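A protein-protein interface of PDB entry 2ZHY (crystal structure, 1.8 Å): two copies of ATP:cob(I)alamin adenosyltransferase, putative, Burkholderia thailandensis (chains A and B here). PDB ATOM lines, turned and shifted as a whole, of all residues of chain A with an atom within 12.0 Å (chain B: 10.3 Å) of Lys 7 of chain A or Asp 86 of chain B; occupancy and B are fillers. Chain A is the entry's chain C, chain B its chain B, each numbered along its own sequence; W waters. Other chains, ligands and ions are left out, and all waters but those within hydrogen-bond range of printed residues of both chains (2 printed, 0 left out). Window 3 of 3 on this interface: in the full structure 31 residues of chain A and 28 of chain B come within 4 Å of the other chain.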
ATOM      1  N   LEU A   5     -15.563  -1.517 -22.794  1.00  0.00           N
ATOM      2  CA  LEU A   5     -16.947  -0.953 -22.824  1.00  0.00           C
ATOM      3  C   LEU A   5     -17.883  -1.943 -23.501  1.00  0.00           C
ATOM      4  O   LEU A   5     -17.783  -2.175 -24.709  1.00  0.00           O
ATOM      5  CB  LEU A   5     -16.972   0.363 -23.606  1.00  0.00           C
ATOM      6  CG  LEU A   5     -17.883   1.487 -23.093  1.00  0.00           C
ATOM      7  CD1 LEU A   5     -18.178   2.448 -24.239  1.00  0.00           C
ATOM      8  CD2 LEU A   5     -19.182   0.919 -22.544  1.00  0.00           C
ATOM      9  N   SER A   6     -18.793  -2.530 -22.732  1.00  0.00           N
ATOM     10  CA  SER A   6     -19.731  -3.496 -23.293  1.00  0.00           C
ATOM     11  C   SER A   6     -20.706  -2.831 -24.257  1.00  0.00           C
ATOM     12  O   SER A   6     -21.232  -1.754 -23.975  1.00  0.00           O
ATOM     13  CB  SER A   6     -20.517  -4.188 -22.178  1.00  0.00           C
ATOM     14  OG  SER A   6     -21.523  -5.021 -22.730  1.00  0.00           O
ATOM     15  N   LYS A   7     -20.949  -3.468 -25.397  1.00  0.00           N
ATOM     16  CA  LYS A   7     -21.879  -2.906 -26.369  1.00  0.00           C
ATOM     17  C   LYS A   7     -23.259  -3.512 -26.149  1.00  0.00           C
ATOM     18  O   LYS A   7     -24.220  -3.165 -26.832  1.00  0.00           O
ATOM     19  CB  LYS A   7     -21.412  -3.183 -27.802  1.00  0.00           C
ATOM     20  CG  LYS A   7     -21.647  -4.609 -28.288  1.00  0.00           C
ATOM     21  CD  LYS A   7     -20.610  -5.579 -27.751  1.00  0.00           C
ATOM     22  CE  LYS A   7     -19.240  -5.328 -28.367  1.00  0.00           C
ATOM     23  NZ  LYS A   7     -18.230  -6.320 -27.894  1.00  0.00           N
ATOM     24  N   ILE A   8     -23.344  -4.420 -25.182  1.00  0.00           N
ATOM     25  CA  ILE A   8     -24.598  -5.088 -24.856  1.00  0.00           C
ATOM     26  C   ILE A   8     -25.460  -4.224 -23.939  1.00  0.00           C
ATOM     27  O   ILE A   8     -25.004  -3.762 -22.890  1.00  0.00           O
ATOM     28  CB  ILE A   8     -24.343  -6.443 -24.154  1.00  0.00           C
ATOM     29  CG1 ILE A   8     -23.582  -7.385 -25.091  1.00  0.00           C
ATOM     30  CG2 ILE A   8     -25.667  -7.069 -23.726  1.00  0.00           C
ATOM     31  CD1 ILE A   8     -24.348  -7.751 -26.348  1.00  0.00           C
ATOM     32  N   ALA A   9     -26.709  -4.011 -24.338  1.00  0.00           N
ATOM     33  CA  ALA A   9     -27.629  -3.217 -23.537  1.00  0.00           C
ATOM     34  C   ALA A   9     -27.834  -3.895 -22.191  1.00  0.00           C
ATOM     35  O   ALA A   9     -27.850  -5.125 -22.099  1.00  0.00           O
ATOM     36  CB  ALA A   9     -28.968  -3.073 -24.258  1.00  0.00           C
ATOM     37  N   THR A  10     -27.989  -3.096 -21.145  1.00  0.00           N
ATOM     38  CA  THR A  10     -28.201  -3.646 -19.818  1.00  0.00           C
ATOM     39  C   THR A  10     -29.653  -4.068 -19.662  1.00  0.00           C
ATOM     40  O   THR A  10     -30.540  -3.529 -20.326  1.00  0.00           O
ATOM     41  CB  THR A  10     -27.891  -2.615 -18.727  1.00  0.00           C
ATOM     42  OG1 THR A  10     -28.871  -1.575 -18.772  1.00  0.00           O
ATOM     43  CG2 THR A  10     -26.515  -2.011 -18.942  1.00  0.00           C
ATOM     44  N   ARG A  11     -29.879  -5.050 -18.796  1.00  0.00           N
ATOM     45  CA  ARG A  11     -31.221  -5.546 -18.506  1.00  0.00           C
ATOM     46  C   ARG A  11     -31.436  -5.300 -17.021  1.00  0.00           C
ATOM     47  O   ARG A  11     -30.470  -5.170 -16.269  1.00  0.00           O
ATOM     48  CB  ARG A  11     -31.325  -7.047 -18.789  1.00  0.00           C
ATOM     49  CG  ARG A  11     -31.465  -7.410 -20.254  1.00  0.00           C
ATOM     50  CD  ARG A  11     -31.204  -8.897 -20.466  1.00  0.00           C
ATOM     51  NE  ARG A  11     -32.094  -9.759 -19.690  1.00  0.00           N
ATOM     52  CZ  ARG A  11     -33.367  -9.997 -19.993  1.00  0.00           C
ATOM     53  NH1 ARG A  11     -33.915  -9.439 -21.065  1.00  0.00           N
ATOM     54  NH2 ARG A  11     -34.090 -10.806 -19.231  1.00  0.00           N
ATOM     55  N   ASP A  14     -29.038  -6.305 -13.953  1.00  0.00           N
ATOM     56  CA  ASP A  14     -27.648  -6.459 -14.368  1.00  0.00           C
ATOM     57  C   ASP A  14     -26.671  -5.889 -13.344  1.00  0.00           C
ATOM     58  O   ASP A  14     -25.538  -6.357 -13.241  1.00  0.00           O
ATOM     59  CB  ASP A  14     -27.400  -5.796 -15.732  1.00  0.00           C
ATOM     60  CG  ASP A  14     -27.666  -6.736 -16.908  1.00  0.00           C
ATOM     61  OD1 ASP A  14     -27.915  -7.940 -16.682  1.00  0.00           O
ATOM     62  OD2 ASP A  14     -27.614  -6.268 -18.067  1.00  0.00           O
ATOM     63  N   ASP B  68     -20.406 -22.541 -21.586  1.00  0.00           N
ATOM     64  CA  ASP B  68     -20.267 -21.184 -21.052  1.00  0.00           C
ATOM     65  C   ASP B  68     -20.060 -21.215 -19.541  1.00  0.00           C
ATOM     66  O   ASP B  68     -19.188 -20.525 -19.014  1.00  0.00           O
ATOM     67  CB  ASP B  68     -21.511 -20.331 -21.334  1.00  0.00           C
ATOM     68  CG  ASP B  68     -21.755 -20.104 -22.814  1.00  0.00           C
ATOM     69  OD1 ASP B  68     -20.826 -20.302 -23.628  1.00  0.00           O
ATOM     70  OD2 ASP B  68     -22.885 -19.706 -23.163  1.00  0.00           O
ATOM     71  N   GLU B  75     -13.334 -18.417 -15.106  1.00  0.00           N
ATOM     72  CA  GLU B  75     -13.037 -17.006 -14.875  1.00  0.00           C
ATOM     73  C   GLU B  75     -13.025 -16.696 -13.377  1.00  0.00           C
ATOM     74  O   GLU B  75     -12.246 -15.866 -12.914  1.00  0.00           O
ATOM     75  CB  GLU B  75     -14.073 -16.118 -15.570  1.00  0.00           C
ATOM     76  CG  GLU B  75     -13.739 -14.627 -15.518  1.00  0.00           C
ATOM     77  CD  GLU B  75     -14.745 -13.768 -16.266  1.00  0.00           C
ATOM     78  OE1 GLU B  75     -15.282 -14.241 -17.292  1.00  0.00           O
ATOM     79  OE2 GLU B  75     -14.985 -12.612 -15.838  1.00  0.00           O
ATOM     80  N   ALA B  82     -10.273 -13.738 -17.831  1.00  0.00           N
ATOM     81  CA  ALA B  82     -11.666 -13.435 -18.121  1.00  0.00           C
ATOM     82  C   ALA B  82     -12.060 -14.373 -19.251  1.00  0.00           C
ATOM     83  O   ALA B  82     -11.202 -14.801 -20.023  1.00  0.00           O
ATOM     84  CB  ALA B  82     -11.807 -11.992 -18.564  1.00  0.00           C
ATOM     85  N   ALA B  83     -13.343 -14.702 -19.352  1.00  0.00           N
ATOM     86  CA  ALA B  83     -13.796 -15.604 -20.403  1.00  0.00           C
ATOM     87  C   ALA B  83     -15.170 -15.236 -20.949  1.00  0.00           C
ATOM     88  O   ALA B  83     -15.459 -15.473 -22.121  1.00  0.00           O
ATOM     89  CB  ALA B  83     -13.810 -17.043 -19.886  1.00  0.00           C
ATOM     90  N   ILE B  84     -16.021 -14.661 -20.106  1.00  0.00           N
ATOM     91  CA  ILE B  84     -17.350 -14.285 -20.565  1.00  0.00           C
ATOM     92  C   ILE B  84     -17.282 -12.904 -21.199  1.00  0.00           C
ATOM     93  O   ILE B  84     -16.830 -11.944 -20.574  1.00  0.00           O
ATOM     94  CB  ILE B  84     -18.368 -14.283 -19.408  1.00  0.00           C
ATOM     95  CG1 ILE B  84     -18.314 -15.625 -18.673  1.00  0.00           C
ATOM     96  CG2 ILE B  84     -19.770 -14.038 -19.951  1.00  0.00           C
ATOM     97  CD1 ILE B  84     -18.513 -16.844 -19.573  1.00  0.00           C
ATOM     98  N   THR B  85     -17.734 -12.817 -22.443  1.00  0.00           N
ATOM     99  CA  THR B  85     -17.711 -11.573 -23.204  1.00  0.00           C
ATOM    100  C   THR B  85     -19.097 -11.172 -23.699  1.00  0.00           C
ATOM    101  O   THR B  85     -20.076 -11.894 -23.486  1.00  0.00           O
ATOM    102  CB  THR B  85     -16.811 -11.719 -24.436  1.00  0.00           C
ATOM    103  OG1 THR B  85     -17.326 -12.765 -25.270  1.00  0.00           O
ATOM    104  CG2 THR B  85     -15.389 -12.065 -24.021  1.00  0.00           C
ATOM    105  N   ASP B  86     -19.171 -10.017 -24.360  1.00  0.00           N
ATOM    106  CA  ASP B  86     -20.437  -9.534 -24.902  1.00  0.00           C
ATOM    107  C   ASP B  86     -21.044 -10.604 -25.797  1.00  0.00           C
ATOM    108  O   ASP B  86     -22.259 -10.753 -25.854  1.00  0.00           O
ATOM    109  CB  ASP B  86     -20.238  -8.261 -25.734  1.00  0.00           C
ATOM    110  CG  ASP B  86     -19.897  -7.047 -24.889  1.00  0.00           C
ATOM    111  OD1 ASP B  86     -20.421  -6.927 -23.763  1.00  0.00           O
ATOM    112  OD2 ASP B  86     -19.115  -6.197 -25.365  1.00  0.00           O
ATOM    113  N   ALA B  87     -20.193 -11.342 -26.501  1.00  0.00           N
ATOM    114  CA  ALA B  87     -20.662 -12.399 -27.397  1.00  0.00           C
ATOM    115  C   ALA B  87     -21.521 -13.400 -26.628  1.00  0.00           C
ATOM    116  O   ALA B  87     -22.573 -13.831 -27.105  1.00  0.00           O
ATOM    117  CB  ALA B  87     -19.472 -13.115 -28.044  1.00  0.00           C
ATOM    118  N   HIS B  88     -21.059 -13.766 -25.438  1.00  0.00           N
ATOM    119  CA  HIS B  88     -21.782 -14.710 -24.596  1.00  0.00           C
ATOM    120  C   HIS B  88     -23.126 -14.118 -24.185  1.00  0.00           C
ATOM    121  O   HIS B  88     -24.141 -14.808 -24.188  1.00  0.00           O
ATOM    122  CB  HIS B  88     -20.959 -15.035 -23.347  1.00  0.00           C
ATOM    123  CG  HIS B  88     -19.668 -15.736 -23.636  1.00  0.00           C
ATOM    124  ND1 HIS B  88     -19.575 -17.105 -23.771  1.00  0.00           N
ATOM    125  CD2 HIS B  88     -18.415 -15.257 -23.816  1.00  0.00           C
ATOM    126  CE1 HIS B  88     -18.321 -17.438 -24.018  1.00  0.00           C
ATOM    127  NE2 HIS B  88     -17.596 -16.334 -24.049  1.00  0.00           N
ATOM    128  N   LEU B  89     -23.127 -12.836 -23.838  1.00  0.00           N
ATOM    129  CA  LEU B  89     -24.354 -12.164 -23.417  1.00  0.00           C
ATOM    130  C   LEU B  89     -25.298 -11.952 -24.593  1.00  0.00           C
ATOM    131  O   LEU B  89     -26.516 -11.992 -24.433  1.00  0.00           O
ATOM    132  CB  LEU B  89     -24.029 -10.816 -22.768  1.00  0.00           C
ATOM    133  CG  LEU B  89     -23.096 -10.856 -21.551  1.00  0.00           C
ATOM    134  CD1 LEU B  89     -22.882  -9.447 -21.021  1.00  0.00           C
ATOM    135  CD2 LEU B  89     -23.697 -11.748 -20.465  1.00  0.00           C
ATOM    136  N   ALA B  90     -24.728 -11.728 -25.773  1.00  0.00           N
ATOM    137  CA  ALA B  90     -25.511 -11.510 -26.981  1.00  0.00           C
ATOM    138  C   ALA B  90     -26.240 -12.786 -27.367  1.00  0.00           C
ATOM    139  O   ALA B  90     -27.397 -12.745 -27.793  1.00  0.00           O
ATOM    140  CB  ALA B  90     -24.602 -11.070 -28.126  1.00  0.00           C
ATOM    141  N   ARG B  91     -25.561 -13.919 -27.221  1.00  0.00           N
ATOM    142  CA  ARG B  91     -26.167 -15.194 -27.571  1.00  0.00           C
ATOM    143  C   ARG B  91     -27.359 -15.475 -26.664  1.00  0.00           C
ATOM    144  O   ARG B  91     -28.391 -15.965 -27.125  1.00  0.00           O
ATOM    145  CB  ARG B  91     -25.142 -16.330 -27.470  1.00  0.00           C
ATOM    146  CG  ARG B  91     -25.648 -17.647 -28.060  1.00  0.00           C
ATOM    147  CD  ARG B  91     -24.513 -18.594 -28.426  1.00  0.00           C
ATOM    148  NE  ARG B  91     -23.753 -19.038 -27.264  1.00  0.00           N
ATOM    149  CZ  ARG B  91     -22.849 -20.011 -27.296  1.00  0.00           C
ATOM    150  NH1 ARG B  91     -22.595 -20.640 -28.436  1.00  0.00           N
ATOM    151  NH2 ARG B  91     -22.201 -20.361 -26.192  1.00  0.00           N
ATOM    152  N   LEU B  92     -27.221 -15.163 -25.378  1.00  0.00           N
ATOM    153  CA  LEU B  92     -28.313 -15.378 -24.435  1.00  0.00           C
ATOM    154  C   LEU B  92     -29.487 -14.483 -24.827  1.00  0.00           C
ATOM    155  O   LEU B  92     -30.619 -14.954 -24.929  1.00  0.00           O
ATOM    156  CB  LEU B  92     -27.873 -15.063 -22.999  1.00  0.00           C
ATOM    157  CG  LEU B  92     -26.836 -15.986 -22.343  1.00  0.00           C
ATOM    158  CD1 LEU B  92     -26.538 -15.486 -20.942  1.00  0.00           C
ATOM    159  CD2 LEU B  92     -27.360 -17.415 -22.283  1.00  0.00           C
ATOM    160  N   ASP B  93     -29.219 -13.195 -25.043  1.00  0.00           N
ATOM    161  CA  ASP B  93     -30.282 -12.276 -25.441  1.00  0.00           C
ATOM    162  C   ASP B  93     -30.955 -12.816 -26.705  1.00  0.00           C
ATOM    163  O   ASP B  93     -32.177 -12.743 -26.851  1.00  0.00           O
ATOM    164  CB  ASP B  93     -29.734 -10.871 -25.723  1.00  0.00           C
ATOM    165  CG  ASP B  93     -29.250 -10.154 -24.467  1.00  0.00           C
ATOM    166  OD1 ASP B  93     -29.648 -10.540 -23.347  1.00  0.00           O
ATOM    167  OD2 ASP B  93     -28.476  -9.181 -24.611  1.00  0.00           O
ATOM    168  N   GLY B  94     -30.152 -13.364 -27.613  1.00  0.00           N
ATOM    169  CA  GLY B  94     -30.689 -13.919 -28.845  1.00  0.00           C
ATOM    170  C   GLY B  94     -31.643 -15.073 -28.581  1.00  0.00           C
ATOM    171  O   GLY B  94     -32.716 -15.146 -29.176  1.00  0.00           O
ATOM    172  N   ASN B 145     -15.506  -8.827 -13.017  1.00  0.00           N
ATOM    173  CA  ASN B 145     -16.057  -8.234 -14.232  1.00  0.00           C
ATOM    174  C   ASN B 145     -17.572  -8.362 -14.093  1.00  0.00           C
ATOM    175  O   ASN B 145     -18.062  -9.216 -13.354  1.00  0.00           O
ATOM    176  CB  ASN B 145     -15.576  -8.988 -15.475  1.00  0.00           C
ATOM    177  CG  ASN B 145     -14.083  -8.848 -15.692  1.00  0.00           C
ATOM    178  OD1 ASN B 145     -13.563  -7.735 -15.767  1.00  0.00           O
ATOM    179  ND2 ASN B 145     -13.383  -9.978 -15.790  1.00  0.00           N
ATOM    180  N   ALA B 146     -18.320  -7.511 -14.781  1.00  0.00           N
ATOM    181  CA  ALA B 146     -19.773  -7.580 -14.689  1.00  0.00           C
ATOM    182  C   ALA B 146     -20.323  -8.766 -15.483  1.00  0.00           C
ATOM    183  O   ALA B 146     -21.369  -9.317 -15.144  1.00  0.00           O
ATOM    184  CB  ALA B 146     -20.386  -6.278 -15.196  1.00  0.00           C
ATOM    185  N   ALA B 147     -19.596  -9.158 -16.524  1.00  0.00           N
ATOM    186  CA  ALA B 147     -19.992 -10.246 -17.414  1.00  0.00           C
ATOM    187  C   ALA B 147     -20.569 -11.502 -16.760  1.00  0.00           C
ATOM    188  O   ALA B 147     -21.654 -11.949 -17.130  1.00  0.00           O
ATOM    189  CB  ALA B 147     -18.815 -10.623 -18.321  1.00  0.00           C
ATOM    190  N   PRO B 148     -19.847 -12.102 -15.799  1.00  0.00           N
ATOM    191  CA  PRO B 148     -20.378 -13.308 -15.155  1.00  0.00           C
ATOM    192  C   PRO B 148     -21.768 -13.071 -14.573  1.00  0.00           C
ATOM    193  O   PRO B 148     -22.696 -13.838 -14.820  1.00  0.00           O
ATOM    194  CB  PRO B 148     -19.343 -13.602 -14.079  1.00  0.00           C
ATOM    195  CG  PRO B 148     -18.070 -13.149 -14.733  1.00  0.00           C
ATOM    196  CD  PRO B 148     -18.482 -11.817 -15.325  1.00  0.00           C
ATOM    197  N   ARG B 150     -23.928 -10.697 -15.283  1.00  0.00           N
ATOM    198  CA  ARG B 150     -24.904 -10.422 -16.329  1.00  0.00           C
ATOM    199  C   ARG B 150     -25.267 -11.677 -17.099  1.00  0.00           C
ATOM    200  O   ARG B 150     -26.364 -11.783 -17.652  1.00  0.00           O
ATOM    201  CB  ARG B 150     -24.363  -9.355 -17.286  1.00  0.00           C
ATOM    202  CG  ARG B 150     -24.123  -7.992 -16.625  1.00  0.00           C
ATOM    203  CD  ARG B 150     -23.515  -6.995 -17.619  1.00  0.00           C
ATOM    204  NE  ARG B 150     -24.448  -6.669 -18.699  1.00  0.00           N
ATOM    205  CZ  ARG B 150     -24.122  -5.998 -19.802  1.00  0.00           C
ATOM    206  NH1 ARG B 150     -22.876  -5.578 -19.990  1.00  0.00           N
ATOM    207  NH2 ARG B 150     -25.047  -5.738 -20.715  1.00  0.00           N
ATOM    208  N   TYR B 151     -24.343 -12.631 -17.140  1.00  0.00           N
ATOM    209  CA  TYR B 151     -24.595 -13.883 -17.840  1.00  0.00           C
ATOM    210  C   TYR B 151     -25.657 -14.700 -17.096  1.00  0.00           C
ATOM    211  O   TYR B 151     -26.682 -15.058 -17.676  1.00  0.00           O
ATOM    212  CB  TYR B 151     -23.309 -14.712 -17.965  1.00  0.00           C
ATOM    213  CG  TYR B 151     -23.494 -15.949 -18.810  1.00  0.00           C
ATOM    214  CD1 TYR B 151     -23.253 -15.920 -20.184  1.00  0.00           C
ATOM    215  CD2 TYR B 151     -23.989 -17.128 -18.251  1.00  0.00           C
ATOM    216  CE1 TYR B 151     -23.511 -17.028 -20.984  1.00  0.00           C
ATOM    217  CE2 TYR B 151     -24.252 -18.242 -19.044  1.00  0.00           C
ATOM    218  CZ  TYR B 151     -24.015 -18.184 -20.408  1.00  0.00           C
ATOM    219  OH  TYR B 151     -24.322 -19.266 -21.198  1.00  0.00           O
ATOM    220  N   ARG B 154     -29.190 -13.259 -17.149  1.00  0.00           N
ATOM    221  CA  ARG B 154     -29.953 -13.562 -18.357  1.00  0.00           C
ATOM    222  C   ARG B 154     -30.326 -15.036 -18.434  1.00  0.00           C
ATOM    223  O   ARG B 154     -31.422 -15.377 -18.876  1.00  0.00           O
ATOM    224  CB  ARG B 154     -29.158 -13.169 -19.606  1.00  0.00           C
ATOM    225  CG  ARG B 154     -29.080 -11.667 -19.842  1.00  0.00           C
ATOM    226  CD  ARG B 154     -28.056 -11.309 -20.909  1.00  0.00           C
ATOM    227  NE  ARG B 154     -28.013  -9.866 -21.115  1.00  0.00           N
ATOM    228  CZ  ARG B 154     -27.665  -8.992 -20.177  1.00  0.00           C
ATOM    229  NH1 ARG B 154     -27.321  -9.419 -18.969  1.00  0.00           N
ATOM    230  NH2 ARG B 154     -27.683  -7.691 -20.442  1.00  0.00           N
HETATM  231  O   HOH W   1     -29.044  -7.298 -22.982  1.00  0.00           O
HETATM  232  O   HOH W   2     -32.304  -9.633 -23.158  1.00  0.00           O
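Of chain B, only Asp 86 and Arg 150 come within 4 Å of Ser 6 of chain A. Of chain B, only Asp 86 comes within 4 Å of Lys 7 of chain A. Ile 8 of chain A touches just these residues of chain B: Asp 86, Ala 90, Asp 93, Arg 150 and Arg 154. Printed residues of chain B within 4 Å of Asp 14 of chain A: Arg 150 and Arg 154. Ala 82 of chain B touches none of the printed residues of chain A. Asp 86 of chain B touches just these residues of chain A: Ser 6 (2.4 Å), Lys 7 (2.7 Å) and Ile 8 (3.5 Å). His 88 of chain B touches none of the printed residues of chain A. No residue of chain A comes within 4 Å of Leu 89 of chain B. Ala 90 of chain B touches one residue of chain A. No residue of chain A comes within 4 Å of Ala 147 of chain B. Of the printed residues of chain A, Arg 154 of chain B touches Ile 8, Ala 9, Arg 11 and Asp 14. The nearest residue of chain B that does not touch Lys 7 of chain A is Ala 87 of chain B (5.6 Å). The nearest printed residue of chain A that does not touch Arg 154 of chain B is Thr 10 of chain A (4.1 Å).
The side-chain carboxylate (OD1) of Asp 86 of chain B sits at hydrogen-bond distance from the side-chain hydroxyl (OG) of Ser 6 of chain A. The guanidinium group of Arg 150 of chain B is in hydrogen-bond range of the backbone carbonyl oxygen of Ile 8 of chain A (2.9 Å). The guanidinium group of Arg 154 of chain B sits at hydrogen-bond distance from the backbone carbonyl oxygen of Ala 9 of chain A, at 3.1 Å. The side-chain carboxylate (OD2) of Asp 86 of chain B is in salt-bridge range of the side-chain amino group (NZ) of Lys 7 of chain A. The guanidinium group (NE) of Arg 150 of chain B lies within salt-bridge range of the side-chain carboxylate (OD2) of Asp 14 of chain A (3.3 Å). NH1 of Arg 150 of chain B lies within hydrogen-bond range of OG of Ser 6 of chain A, 3.1 Å away. The guanidinium group (NH2) of Arg 150 of chain B lies within hydrogen-bond range of the backbone carbonyl oxygen (O) of Ala 9 of chain A (3.2 Å). The guanidinium group (NH2) of Arg 154 of chain B lies within salt-bridge range of the side-chain carboxylate (OD2) of Asp 14 of chain A, 2.8 Å away.
Ile 8 of chain A touches Asp 86 of chain B (CG1 to OD1, 3.5 Å). Ala 90 of chain B touches Ile 8 of chain A. Asp 93 of chain B touches Ile 8 of chain A (OD2 to CG2, 3.6 Å). Ile 8 of chain A touches Arg 154 of chain B (CG2 to NH2, 3.9 Å). Arg 150 of chain B touches Thr 10 of chain A (NH2 to CA, 3.9 Å). Asp 93 of chain B touches Arg 11 of chain A. Arg 11 of chain A touches Arg 154 of chain B (CD to NE, 3.4 Å).
Water W1 lies within hydrogen-bond range of the side-chain carboxylate (OD2) of Asp 93 of chain B (2.6 Å), the backbone carbonyl oxygen (O) of Ala 9 of chain A (2.6 Å) and the guanidinium group (NH2) of Arg 154 of chain B (2.9 Å). Water W2 lies within hydrogen-bond range of the guanidinium group (NH1) of Arg 11 of chain A (2.6 Å) and the side-chain carboxylate (OD1) of Asp 93 of chain B (2.8 Å).
No position is printed for both chains. Of the 15 pairs that touch across the chains among the printed residues, none has its exchanged pair printed and touching as well.
Printed residues of chain A that touch a printed residue of chain B: Ser 6, Lys 7, Ile 8, Ala 9, Thr 10, Arg 11 and Asp 14. Hydrophobic or aromatic side chains of chain A that line the printed part of chain B: Ile 8. Along chain A the printed residues that touch a printed residue of chain B span positions 6 to 14. Of the 22 printed residues of chain B, 5 touch a printed residue of chain A. Hydrophobic or aromatic side chains of chain B that line the printed part of chain A: Ala 90. Among the printed residues, Asp or Glu carboxylates within 4 Å of a Lys or Arg side-chain nitrogen of the other chain: Lys 7 of chain A with Asp 86 of chain B, Asp 14 of chain A with Arg 150 of chain B and Asp 14 of chain A with Arg 154 of chain B.
The guanidinium group (NE) of Arg 154 of chain B is in salt-bridge range of the side-chain carboxylate (OD1) of Asp 93 of chain B. The backbone carbonyl oxygen of Arg 150 of chain B sits at hydrogen-bond distance from the guanidinium group of Arg 154 of chain B. OD2 of Asp 14 of chain A sits at hydrogen-bond distance from N of Arg 11 of chain A. OG of Ser 6 of chain A is in hydrogen-bond range of N of Ile 8 of chain A (3.1 Å).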
